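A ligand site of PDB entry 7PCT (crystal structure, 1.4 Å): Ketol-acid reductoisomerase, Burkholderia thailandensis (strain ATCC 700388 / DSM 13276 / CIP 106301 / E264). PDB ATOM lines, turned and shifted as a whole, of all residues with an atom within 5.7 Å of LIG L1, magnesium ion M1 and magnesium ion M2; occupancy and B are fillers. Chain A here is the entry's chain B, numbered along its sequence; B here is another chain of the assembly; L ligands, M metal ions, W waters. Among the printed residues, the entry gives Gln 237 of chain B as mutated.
Water W2 lies within hydrogen-bond range of OE1 of Glu 231 of chain B (2.7 Å), OE1 of Gln 237 of chain B (2.8 Å) and NH2 of Arg 136 (3.2 Å).
Water W3 bridges O of Pro 135 and NH1 of Arg 136.
Water W4 lies within hydrogen-bond range of the side-chain amide oxygen of Gln 199 (2.6 Å) and the side-chain amide nitrogen of Gln 237 of chain B (3.3 Å).
Water W5 bridges OE1 of Glu 200 (2.7 Å) and NE2 of His 113 (3.2 Å).
Merely in contact with magnesium ion M1: Arg 136 (3.9 Å) and Gln 237 of chain B (3.99 Å).
Of the 19 residues printed, 4 come within 4 Å of magnesium ion M1.
Merely in contact with LIG L1: Cys 262 of chain B (3.3 Å), Met 137 (3.3 Å), Gly 258 of chain B (3.5 Å) and Pro 135 (3.96 Å).
Of the 19 residues printed, 9 come within 4 Å of LIG L1.
The nearest printed residue that does not touch LIG L1 is Gln 257 of chain B (4.1 Å).
O2 of LIG L1 lies within hydrogen-bond range of N7 of LG2 L2.
O9 of LG2 L2 sits at hydrogen-bond distance from N of Gln 34 (3.0 Å).
N of Ser 259 of chain B sits at hydrogen-bond distance from O2 of LIG L1.
An oxygen (O12) of LG2 L2 lies within hydrogen-bond range of the side-chain carboxylate of Asp 88, 2.6 Å away.
N7 of LG2 L2 sits at hydrogen-bond distance from O of Gln 257 of chain B.
OG of Ser 259 of chain B lies within hydrogen-bond range of O2 of LIG L1.
The backbone NH (N) of Tyr 138 lies within hydrogen-bond range of an oxygen (O4) of LIG L1 (3.4 Å).
The side-chain amide nitrogen (NE2) of Gln 34 is in hydrogen-bond range of an oxygen (O14) of LG2 L2.
NE2 of Gln 237 of chain B is in hydrogen-bond range of O4 of LIG L1 (2.9 Å).
The side-chain carboxylate (OD1) of Asp 196 binds magnesium ion M1 (2.0 Å).
Magnesium ion M1 is bound by an oxygen (O5) of LIG L1 (2.1 Å).
Water W2 is bound to magnesium ion M1, 2.1 Å away.
O3 of LIG L1 binds magnesium ion M1.
Water W3 is bound to magnesium ion M1 (2.1 Å).
Magnesium ion M1 is bound by water W4, 2.1 Å away.
Magnesium ion M1 has six donor atoms within binding distance.
OD2 of Asp 196 binds magnesium ion M2, at 2.0 Å.
Magnesium ion M2 is bound by OE2 of Glu 200, 2.1 Å away.
Magnesium ion M2 is bound by water W1, 2.1 Å away.
Water W5 is bound to magnesium ion M2.
Magnesium ion M2 is bound by O1 of LIG L1 (2.1 Å).
O3 of LIG L1 binds magnesium ion M2 (2.1 Å).
Magnesium ion M2 has six donor atoms within binding distance.
NE2 of Gln 34 is in hydrogen-bond range of O of Met 137 (3.0 Å).
The guanidinium group (NE) of Arg 136 lies within salt-bridge range of the side-chain carboxylate (OE2) of Glu 231 of chain B (2.8 Å).
OD1 of Asp 196 sits close to NH2 of Arg 136.
The side-chain amide oxygen of Gln 237 of chain B sits at hydrogen-bond distance from the side-chain amide nitrogen of Gln 199.
OE2 of Glu 192 is in salt-bridge range of NH1 of Arg 136, 2.8 Å away.
The side-chain hydroxyl of Ser 259 of chain B lies within hydrogen-bond range of the backbone NH of Cys 262 of chain B.
The side-chain hydroxyl (OG) of Ser 259 of chain B lies close to the backbone NH (N) of Thr 261 of chain B (3.4 Å).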
ATOM      1  N   GLN A  34       9.905 -19.007 -13.786  1.00  0.00           N
ATOM      2  CA  GLN A  34      10.755 -20.213 -13.686  1.00  0.00           C
ATOM      3  C   GLN A  34      11.626 -20.166 -12.420  1.00  0.00           C
ATOM      4  O   GLN A  34      11.671 -21.167 -11.688  1.00  0.00           O
ATOM      5  CB  GLN A  34      11.591 -20.385 -14.956  1.00  0.00           C
ATOM      6  CG  GLN A  34      10.748 -20.807 -16.150  1.00  0.00           C
ATOM      7  CD  GLN A  34      10.128 -22.168 -15.944  1.00  0.00           C
ATOM      8  OE1 GLN A  34      10.752 -23.081 -15.414  1.00  0.00           O
ATOM      9  NE2 GLN A  34       8.865 -22.313 -16.337  1.00  0.00           N
ATOM     10  N   ASP A  88      15.223 -13.402 -21.727  1.00  0.00           N
ATOM     11  CA  ASP A  88      16.280 -13.784 -22.700  1.00  0.00           C
ATOM     12  C   ASP A  88      17.016 -12.532 -23.215  1.00  0.00           C
ATOM     13  O   ASP A  88      18.248 -12.608 -23.366  1.00  0.00           O
ATOM     14  CB  ASP A  88      15.638 -14.596 -23.817  1.00  0.00           C
ATOM     15  CG  ASP A  88      14.906 -15.786 -23.220  1.00  0.00           C
ATOM     16  OD1 ASP A  88      15.599 -16.767 -22.887  1.00  0.00           O
ATOM     17  OD2 ASP A  88      13.671 -15.680 -23.011  1.00  0.00           O
ATOM     18  N   HIS A 113      16.155 -21.780 -22.193  1.00  0.00           N
ATOM     19  CA  HIS A 113      15.697 -21.478 -23.572  1.00  0.00           C
ATOM     20  C   HIS A 113      16.943 -21.251 -24.412  1.00  0.00           C
ATOM     21  O   HIS A 113      17.893 -20.623 -23.912  1.00  0.00           O
ATOM     22  CB  HIS A 113      14.781 -20.239 -23.548  1.00  0.00           C
ATOM     23  CG  HIS A 113      14.175 -19.789 -24.857  1.00  0.00           C
ATOM     24  ND1 HIS A 113      13.686 -20.655 -25.837  1.00  0.00           N
ATOM     25  CD2 HIS A 113      13.818 -18.547 -25.264  1.00  0.00           C
ATOM     26  CE1 HIS A 113      13.144 -19.945 -26.805  1.00  0.00           C
ATOM     27  NE2 HIS A 113      13.213 -18.647 -26.477  1.00  0.00           N
ATOM     28  N   PRO A 135      12.189 -26.269 -19.524  1.00  0.00           N
ATOM     29  CA  PRO A 135      10.907 -26.869 -19.154  1.00  0.00           C
ATOM     30  C   PRO A 135       9.823 -26.608 -20.204  1.00  0.00           C
ATOM     31  O   PRO A 135       9.867 -25.558 -20.855  1.00  0.00           O
ATOM     32  CB  PRO A 135      10.549 -26.168 -17.824  1.00  0.00           C
ATOM     33  CG  PRO A 135      11.876 -25.678 -17.312  1.00  0.00           C
ATOM     34  CD  PRO A 135      12.616 -25.235 -18.554  1.00  0.00           C
ATOM     35  N   ARG A 136       8.864 -27.521 -20.330  1.00  0.00           N
ATOM     36  CA  ARG A 136       7.745 -27.384 -21.301  1.00  0.00           C
ATOM     37  C   ARG A 136       6.469 -26.994 -20.546  1.00  0.00           C
ATOM     38  O   ARG A 136       5.374 -27.434 -20.935  1.00  0.00           O
ATOM     39  CB  ARG A 136       7.513 -28.684 -22.085  1.00  0.00           C
ATOM     40  CG  ARG A 136       8.760 -29.348 -22.631  1.00  0.00           C
ATOM     41  CD  ARG A 136       9.814 -28.390 -23.148  1.00  0.00           C
ATOM     42  NE  ARG A 136       9.378 -27.456 -24.177  1.00  0.00           N
ATOM     43  CZ  ARG A 136      10.133 -26.463 -24.632  1.00  0.00           C
ATOM     44  NH1 ARG A 136      11.319 -26.234 -24.098  1.00  0.00           N
ATOM     45  NH2 ARG A 136       9.700 -25.699 -25.623  1.00  0.00           N
ATOM     46  N   MET A 137       6.602 -26.185 -19.512  1.00  0.00           N
ATOM     47  CA  MET A 137       5.469 -25.797 -18.641  1.00  0.00           C
ATOM     48  C   MET A 137       5.877 -24.560 -17.857  1.00  0.00           C
ATOM     49  O   MET A 137       7.082 -24.356 -17.663  1.00  0.00           O
ATOM     50  CB  MET A 137       5.181 -26.955 -17.687  1.00  0.00           C
ATOM     51  CG  MET A 137       4.020 -26.747 -16.746  1.00  0.00           C
ATOM     52  SD  MET A 137       2.475 -26.401 -17.636  1.00  0.00           S
ATOM     53  CE  MET A 137       2.361 -27.878 -18.647  1.00  0.00           C
ATOM     54  N   TYR A 138       4.903 -23.766 -17.411  1.00  0.00           N
ATOM     55  CA  TYR A 138       5.176 -22.564 -16.601  1.00  0.00           C
ATOM     56  C   TYR A 138       5.263 -22.967 -15.116  1.00  0.00           C
ATOM     57  O   TYR A 138       5.084 -24.145 -14.781  1.00  0.00           O
ATOM     58  CB  TYR A 138       4.226 -21.419 -16.946  1.00  0.00           C
ATOM     59  CG  TYR A 138       2.748 -21.709 -17.050  1.00  0.00           C
ATOM     60  CD1 TYR A 138       1.911 -21.532 -15.967  1.00  0.00           C
ATOM     61  CD2 TYR A 138       2.193 -22.076 -18.261  1.00  0.00           C
ATOM     62  CE1 TYR A 138       0.543 -21.751 -16.070  1.00  0.00           C
ATOM     63  CE2 TYR A 138       0.829 -22.296 -18.388  1.00  0.00           C
ATOM     64  CZ  TYR A 138       0.002 -22.127 -17.295  1.00  0.00           C
ATOM     65  OH  TYR A 138      -1.344 -22.334 -17.456  1.00  0.00           O
ATOM     66  N   GLU A 192      15.228 -26.194 -30.037  1.00  0.00           N
ATOM     67  CA  GLU A 192      14.343 -25.794 -28.910  1.00  0.00           C
ATOM     68  C   GLU A 192      13.889 -24.355 -29.132  1.00  0.00           C
ATOM     69  O   GLU A 192      12.708 -24.055 -28.910  1.00  0.00           O
ATOM     70  CB  GLU A 192      15.054 -25.938 -27.568  1.00  0.00           C
ATOM     71  CG  GLU A 192      14.132 -25.733 -26.386  1.00  0.00           C
ATOM     72  CD  GLU A 192      13.797 -24.304 -25.972  1.00  0.00           C
ATOM     73  OE1 GLU A 192      14.595 -23.382 -26.256  1.00  0.00           O
ATOM     74  OE2 GLU A 192      12.745 -24.137 -25.321  1.00  0.00           O
ATOM     75  N   ASP A 196       9.924 -23.580 -29.526  1.00  0.00           N
ATOM     76  CA  ASP A 196       9.316 -22.802 -28.416  1.00  0.00           C
ATOM     77  C   ASP A 196       8.668 -21.527 -28.976  1.00  0.00           C
ATOM     78  O   ASP A 196       7.500 -21.210 -28.636  1.00  0.00           O
ATOM     79  CB  ASP A 196      10.379 -22.504 -27.349  1.00  0.00           C
ATOM     80  CG  ASP A 196       9.779 -22.016 -26.053  1.00  0.00           C
ATOM     81  OD1 ASP A 196       8.976 -22.783 -25.462  1.00  0.00           O
ATOM     82  OD2 ASP A 196      10.052 -20.867 -25.686  1.00  0.00           O
ATOM     83  N   LEU A 197       9.408 -20.778 -29.781  1.00  0.00           N
ATOM     84  CA  LEU A 197       8.919 -19.482 -30.317  1.00  0.00           C
ATOM     85  C   LEU A 197       7.719 -19.745 -31.235  1.00  0.00           C
ATOM     86  O   LEU A 197       6.776 -18.942 -31.226  1.00  0.00           O
ATOM     87  CB  LEU A 197      10.053 -18.757 -31.064  1.00  0.00           C
ATOM     88  CG  LEU A 197      11.219 -18.279 -30.190  1.00  0.00           C
ATOM     89  CD1 LEU A 197      12.276 -17.607 -31.053  1.00  0.00           C
ATOM     90  CD2 LEU A 197      10.758 -17.332 -29.087  1.00  0.00           C
ATOM     91  N   GLN A 199       5.401 -22.156 -30.935  1.00  0.00           N
ATOM     92  CA  GLN A 199       4.240 -22.391 -30.042  1.00  0.00           C
ATOM     93  C   GLN A 199       3.700 -21.037 -29.568  1.00  0.00           C
ATOM     94  O   GLN A 199       2.479 -20.859 -29.520  1.00  0.00           O
ATOM     95  CB  GLN A 199       4.672 -23.268 -28.862  1.00  0.00           C
ATOM     96  CG  GLN A 199       3.521 -23.745 -28.004  1.00  0.00           C
ATOM     97  CD  GLN A 199       3.928 -23.872 -26.563  1.00  0.00           C
ATOM     98  OE1 GLN A 199       4.426 -22.932 -25.960  1.00  0.00           O
ATOM     99  NE2 GLN A 199       3.685 -25.044 -25.995  1.00  0.00           N
ATOM    100  N   GLU A 200       4.587 -20.104 -29.264  1.00  0.00           N
ATOM    101  CA  GLU A 200       4.225 -18.798 -28.653  1.00  0.00           C
ATOM    102  C   GLU A 200       3.623 -17.853 -29.699  1.00  0.00           C
ATOM    103  O   GLU A 200       2.811 -16.978 -29.312  1.00  0.00           O
ATOM    104  CB  GLU A 200       5.442 -18.173 -27.989  1.00  0.00           C
ATOM    105  CG  GLU A 200       5.924 -18.975 -26.802  1.00  0.00           C
ATOM    106  CD  GLU A 200       7.298 -18.667 -26.269  1.00  0.00           C
ATOM    107  OE1 GLU A 200       7.991 -17.815 -26.857  1.00  0.00           O
ATOM    108  OE2 GLU A 200       7.666 -19.287 -25.231  1.00  0.00           O
ATOM    109  N   GLU B 231       4.718 -29.822 -27.752  1.00  0.00           N
ATOM    110  CA  GLU B 231       4.492 -28.359 -27.755  1.00  0.00           C
ATOM    111  C   GLU B 231       3.041 -28.061 -28.133  1.00  0.00           C
ATOM    112  O   GLU B 231       2.456 -27.154 -27.549  1.00  0.00           O
ATOM    113  CB  GLU B 231       5.467 -27.650 -28.675  1.00  0.00           C
ATOM    114  CG  GLU B 231       6.896 -27.788 -28.209  1.00  0.00           C
ATOM    115  CD  GLU B 231       7.119 -27.412 -26.763  1.00  0.00           C
ATOM    116  OE1 GLU B 231       6.989 -26.218 -26.457  1.00  0.00           O
ATOM    117  OE2 GLU B 231       7.402 -28.314 -25.950  1.00  0.00           O
ATOM    118  N   GLN B 237       0.789 -27.903 -21.666  1.00  0.00           N
ATOM    119  CA  GLN B 237       0.917 -26.429 -21.539  1.00  0.00           C
ATOM    120  C   GLN B 237      -0.281 -25.739 -22.188  1.00  0.00           C
ATOM    121  O   GLN B 237      -0.821 -24.792 -21.584  1.00  0.00           O
ATOM    122  CB  GLN B 237       2.233 -25.929 -22.128  1.00  0.00           C
ATOM    123  CG  GLN B 237       2.483 -24.446 -21.885  1.00  0.00           C
ATOM    124  CD  GLN B 237       3.684 -23.949 -22.660  1.00  0.00           C
ATOM    125  OE1 GLN B 237       4.547 -24.730 -23.052  1.00  0.00           O
ATOM    126  NE2 GLN B 237       3.750 -22.635 -22.856  1.00  0.00           N
ATOM    127  N   GLN B 257       2.007 -15.439 -17.033  1.00  0.00           N
ATOM    128  CA  GLN B 257       2.808 -16.689 -17.020  1.00  0.00           C
ATOM    129  C   GLN B 257       3.829 -16.731 -18.155  1.00  0.00           C
ATOM    130  O   GLN B 257       4.644 -17.660 -18.159  1.00  0.00           O
ATOM    131  CB  GLN B 257       1.914 -17.921 -17.110  1.00  0.00           C
ATOM    132  CG  GLN B 257       0.883 -17.983 -15.999  1.00  0.00           C
ATOM    133  CD  GLN B 257       1.447 -18.314 -14.638  1.00  0.00           C
ATOM    134  OE1 GLN B 257       2.626 -18.112 -14.353  1.00  0.00           O
ATOM    135  NE2 GLN B 257       0.592 -18.863 -13.791  1.00  0.00           N
ATOM    136  N   GLY B 258       3.783 -15.785 -19.089  1.00  0.00           N
ATOM    137  CA  GLY B 258       4.724 -15.787 -20.215  1.00  0.00           C
ATOM    138  C   GLY B 258       5.982 -15.002 -19.884  1.00  0.00           C
ATOM    139  O   GLY B 258       5.879 -13.909 -19.267  1.00  0.00           O
ATOM    140  N   SER B 259       7.143 -15.500 -20.312  1.00  0.00           N
ATOM    141  CA  SER B 259       8.386 -14.701 -20.319  1.00  0.00           C
ATOM    142  C   SER B 259       8.126 -13.462 -21.174  1.00  0.00           C
ATOM    143  O   SER B 259       7.246 -13.463 -22.032  1.00  0.00           O
ATOM    144  CB  SER B 259       9.551 -15.486 -20.853  1.00  0.00           C
ATOM    145  OG  SER B 259       9.424 -15.668 -22.269  1.00  0.00           O
ATOM    146  N   THR B 261       9.827 -12.631 -23.726  1.00  0.00           N
ATOM    147  CA  THR B 261      10.026 -13.196 -25.075  1.00  0.00           C
ATOM    148  C   THR B 261       8.710 -13.774 -25.580  1.00  0.00           C
ATOM    149  O   THR B 261       8.306 -13.489 -26.708  1.00  0.00           O
ATOM    150  CB  THR B 261      11.088 -14.297 -25.064  1.00  0.00           C
ATOM    151  OG1 THR B 261      12.249 -13.739 -24.442  1.00  0.00           O
ATOM    152  CG2 THR B 261      11.399 -14.803 -26.445  1.00  0.00           C
ATOM    153  N   CYS B 262       8.053 -14.577 -24.742  1.00  0.00           N
ATOM    154  CA  CYS B 262       6.760 -15.202 -25.079  1.00  0.00           C
ATOM    155  C   CYS B 262       5.702 -14.120 -25.305  1.00  0.00           C
ATOM    156  O   CYS B 262       4.983 -14.193 -26.303  1.00  0.00           O
ATOM    157  CB  CYS B 262       6.336 -16.105 -23.927  1.00  0.00           C
ATOM    158  SG  CYS B 262       4.642 -16.711 -24.088  1.00  0.00           S
HETATM  159  C1  LIG L   1       7.952 -18.725 -22.098  1.00  0.00           C
HETATM  160  O1  LIG L   1       8.876 -18.224 -22.786  1.00  0.00           O
HETATM  161  C2  LIG L   1       7.755 -20.186 -22.192  1.00  0.00           C
HETATM  162  O2  LIG L   1       7.188 -18.035 -21.375  1.00  0.00           O
HETATM  163  C3  LIG L   1       6.652 -20.747 -21.397  1.00  0.00           C
HETATM  164  O3  LIG L   1       8.510 -20.911 -23.044  1.00  0.00           O
HETATM  165  C4  LIG L   1       6.352 -22.231 -21.293  1.00  0.00           C
HETATM  166  O4  LIG L   1       5.438 -22.547 -20.487  1.00  0.00           O
HETATM  167  O5  LIG L   1       6.971 -23.104 -21.967  1.00  0.00           O
HETATM  168  P1  LG2 L   2      10.179 -13.502 -15.807  1.00  0.00           P
HETATM  169  O1  LG2 L   2       9.617 -12.412 -16.638  1.00  0.00           O
HETATM  170  O2  LG2 L   2       9.294 -14.126 -14.794  1.00  0.00           O
HETATM  171  O3  LG2 L   2      11.538 -13.032 -15.143  1.00  0.00           O
HETATM  172  C1  LG2 L   2      11.522 -12.109 -14.051  1.00  0.00           C
HETATM  173  C2  LG2 L   2      12.833 -12.263 -13.337  1.00  0.00           C
HETATM  174  O4  LG2 L   2      13.893 -11.754 -14.183  1.00  0.00           O
HETATM  175  C3  LG2 L   2      12.970 -11.510 -12.010  1.00  0.00           C
HETATM  176  O5  LG2 L   2      13.785 -12.249 -11.109  1.00  0.00           O
HETATM  177  C4  LG2 L   2      13.626 -10.201 -12.453  1.00  0.00           C
HETATM  178  O6  LG2 L   2      14.303  -9.608 -11.383  1.00  0.00           O
HETATM  179  C5  LG2 L   2      14.578 -10.719 -13.520  1.00  0.00           C
HETATM  180  N1  LG2 L   2      14.978  -9.706 -14.492  1.00  0.00           N
HETATM  181  C6  LG2 L   2      14.173  -9.020 -15.373  1.00  0.00           C
HETATM  182  N2  LG2 L   2      14.853  -8.183 -16.116  1.00  0.00           N
HETATM  183  C7  LG2 L   2      16.163  -8.309 -15.714  1.00  0.00           C
HETATM  184  C8  LG2 L   2      17.360  -7.684 -16.111  1.00  0.00           C
HETATM  185  N3  LG2 L   2      17.439  -6.755 -17.060  1.00  0.00           N
HETATM  186  N4  LG2 L   2      18.503  -8.064 -15.488  1.00  0.00           N
HETATM  187  C9  LG2 L   2      18.429  -8.995 -14.526  1.00  0.00           C
HETATM  188  N5  LG2 L   2      17.362  -9.647 -14.071  1.00  0.00           N
HETATM  189  C10 LG2 L   2      16.261  -9.267 -14.716  1.00  0.00           C
HETATM  190  O7  LG2 L   2      10.797 -14.618 -16.775  1.00  0.00           O
HETATM  191  P2  LG2 L   2      10.610 -16.199 -16.947  1.00  0.00           P
HETATM  192  O8  LG2 L   2       9.362 -16.416 -17.738  1.00  0.00           O
HETATM  193  O9  LG2 L   2      10.751 -16.853 -15.625  1.00  0.00           O
HETATM  194  O10 LG2 L   2      11.844 -16.554 -17.909  1.00  0.00           O
HETATM  195  C11 LG2 L   2      13.155 -16.899 -17.414  1.00  0.00           C
HETATM  196  C12 LG2 L   2      13.804 -17.788 -18.431  1.00  0.00           C
HETATM  197  O11 LG2 L   2      13.038 -19.014 -18.519  1.00  0.00           O
HETATM  198  C13 LG2 L   2      13.866 -17.260 -19.875  1.00  0.00           C
HETATM  199  O12 LG2 L   2      15.057 -17.744 -20.485  1.00  0.00           O
HETATM  200  C14 LG2 L   2      12.633 -17.894 -20.513  1.00  0.00           C
HETATM  201  O13 LG2 L   2      12.729 -18.025 -21.924  1.00  0.00           O
HETATM  202  C15 LG2 L   2      12.675 -19.263 -19.856  1.00  0.00           C
HETATM  203  N6  LG2 L   2      11.396 -20.028 -19.840  1.00  0.00           N
HETATM  204  C16 LG2 L   2      10.230 -19.488 -19.359  1.00  0.00           C
HETATM  205  C17 LG2 L   2       9.127 -20.279 -19.128  1.00  0.00           C
HETATM  206  C18 LG2 L   2       7.888 -19.751 -18.519  1.00  0.00           C
HETATM  207  O14 LG2 L   2       7.022 -20.571 -18.191  1.00  0.00           O
HETATM  208  N7  LG2 L   2       7.718 -18.447 -18.342  1.00  0.00           N
HETATM  209  C19 LG2 L   2       9.197 -21.719 -19.460  1.00  0.00           C
HETATM  210  C20 LG2 L   2      10.477 -22.189 -19.963  1.00  0.00           C
HETATM  211  C21 LG2 L   2      11.446 -21.341 -20.232  1.00  0.00           C
HETATM  212 MG    MG M   1       7.970 -22.809 -23.745  1.00  0.00          MG
HETATM  213 MG    MG M   2       9.501 -19.524 -24.321  1.00  0.00          MG
HETATM  214  O   HOH W   1      11.263 -19.911 -23.301  1.00  0.00           O
HETATM  215  O   HOH W   2       7.021 -24.596 -24.248  1.00  0.00           O
HETATM  216  O   HOH W   3       9.679 -23.681 -22.872  1.00  0.00           O
HETATM  217  O   HOH W   4       6.372 -21.758 -24.656  1.00  0.00           O
HETATM  218  O   HOH W   5      10.321 -17.966 -25.421  1.00  0.00           O
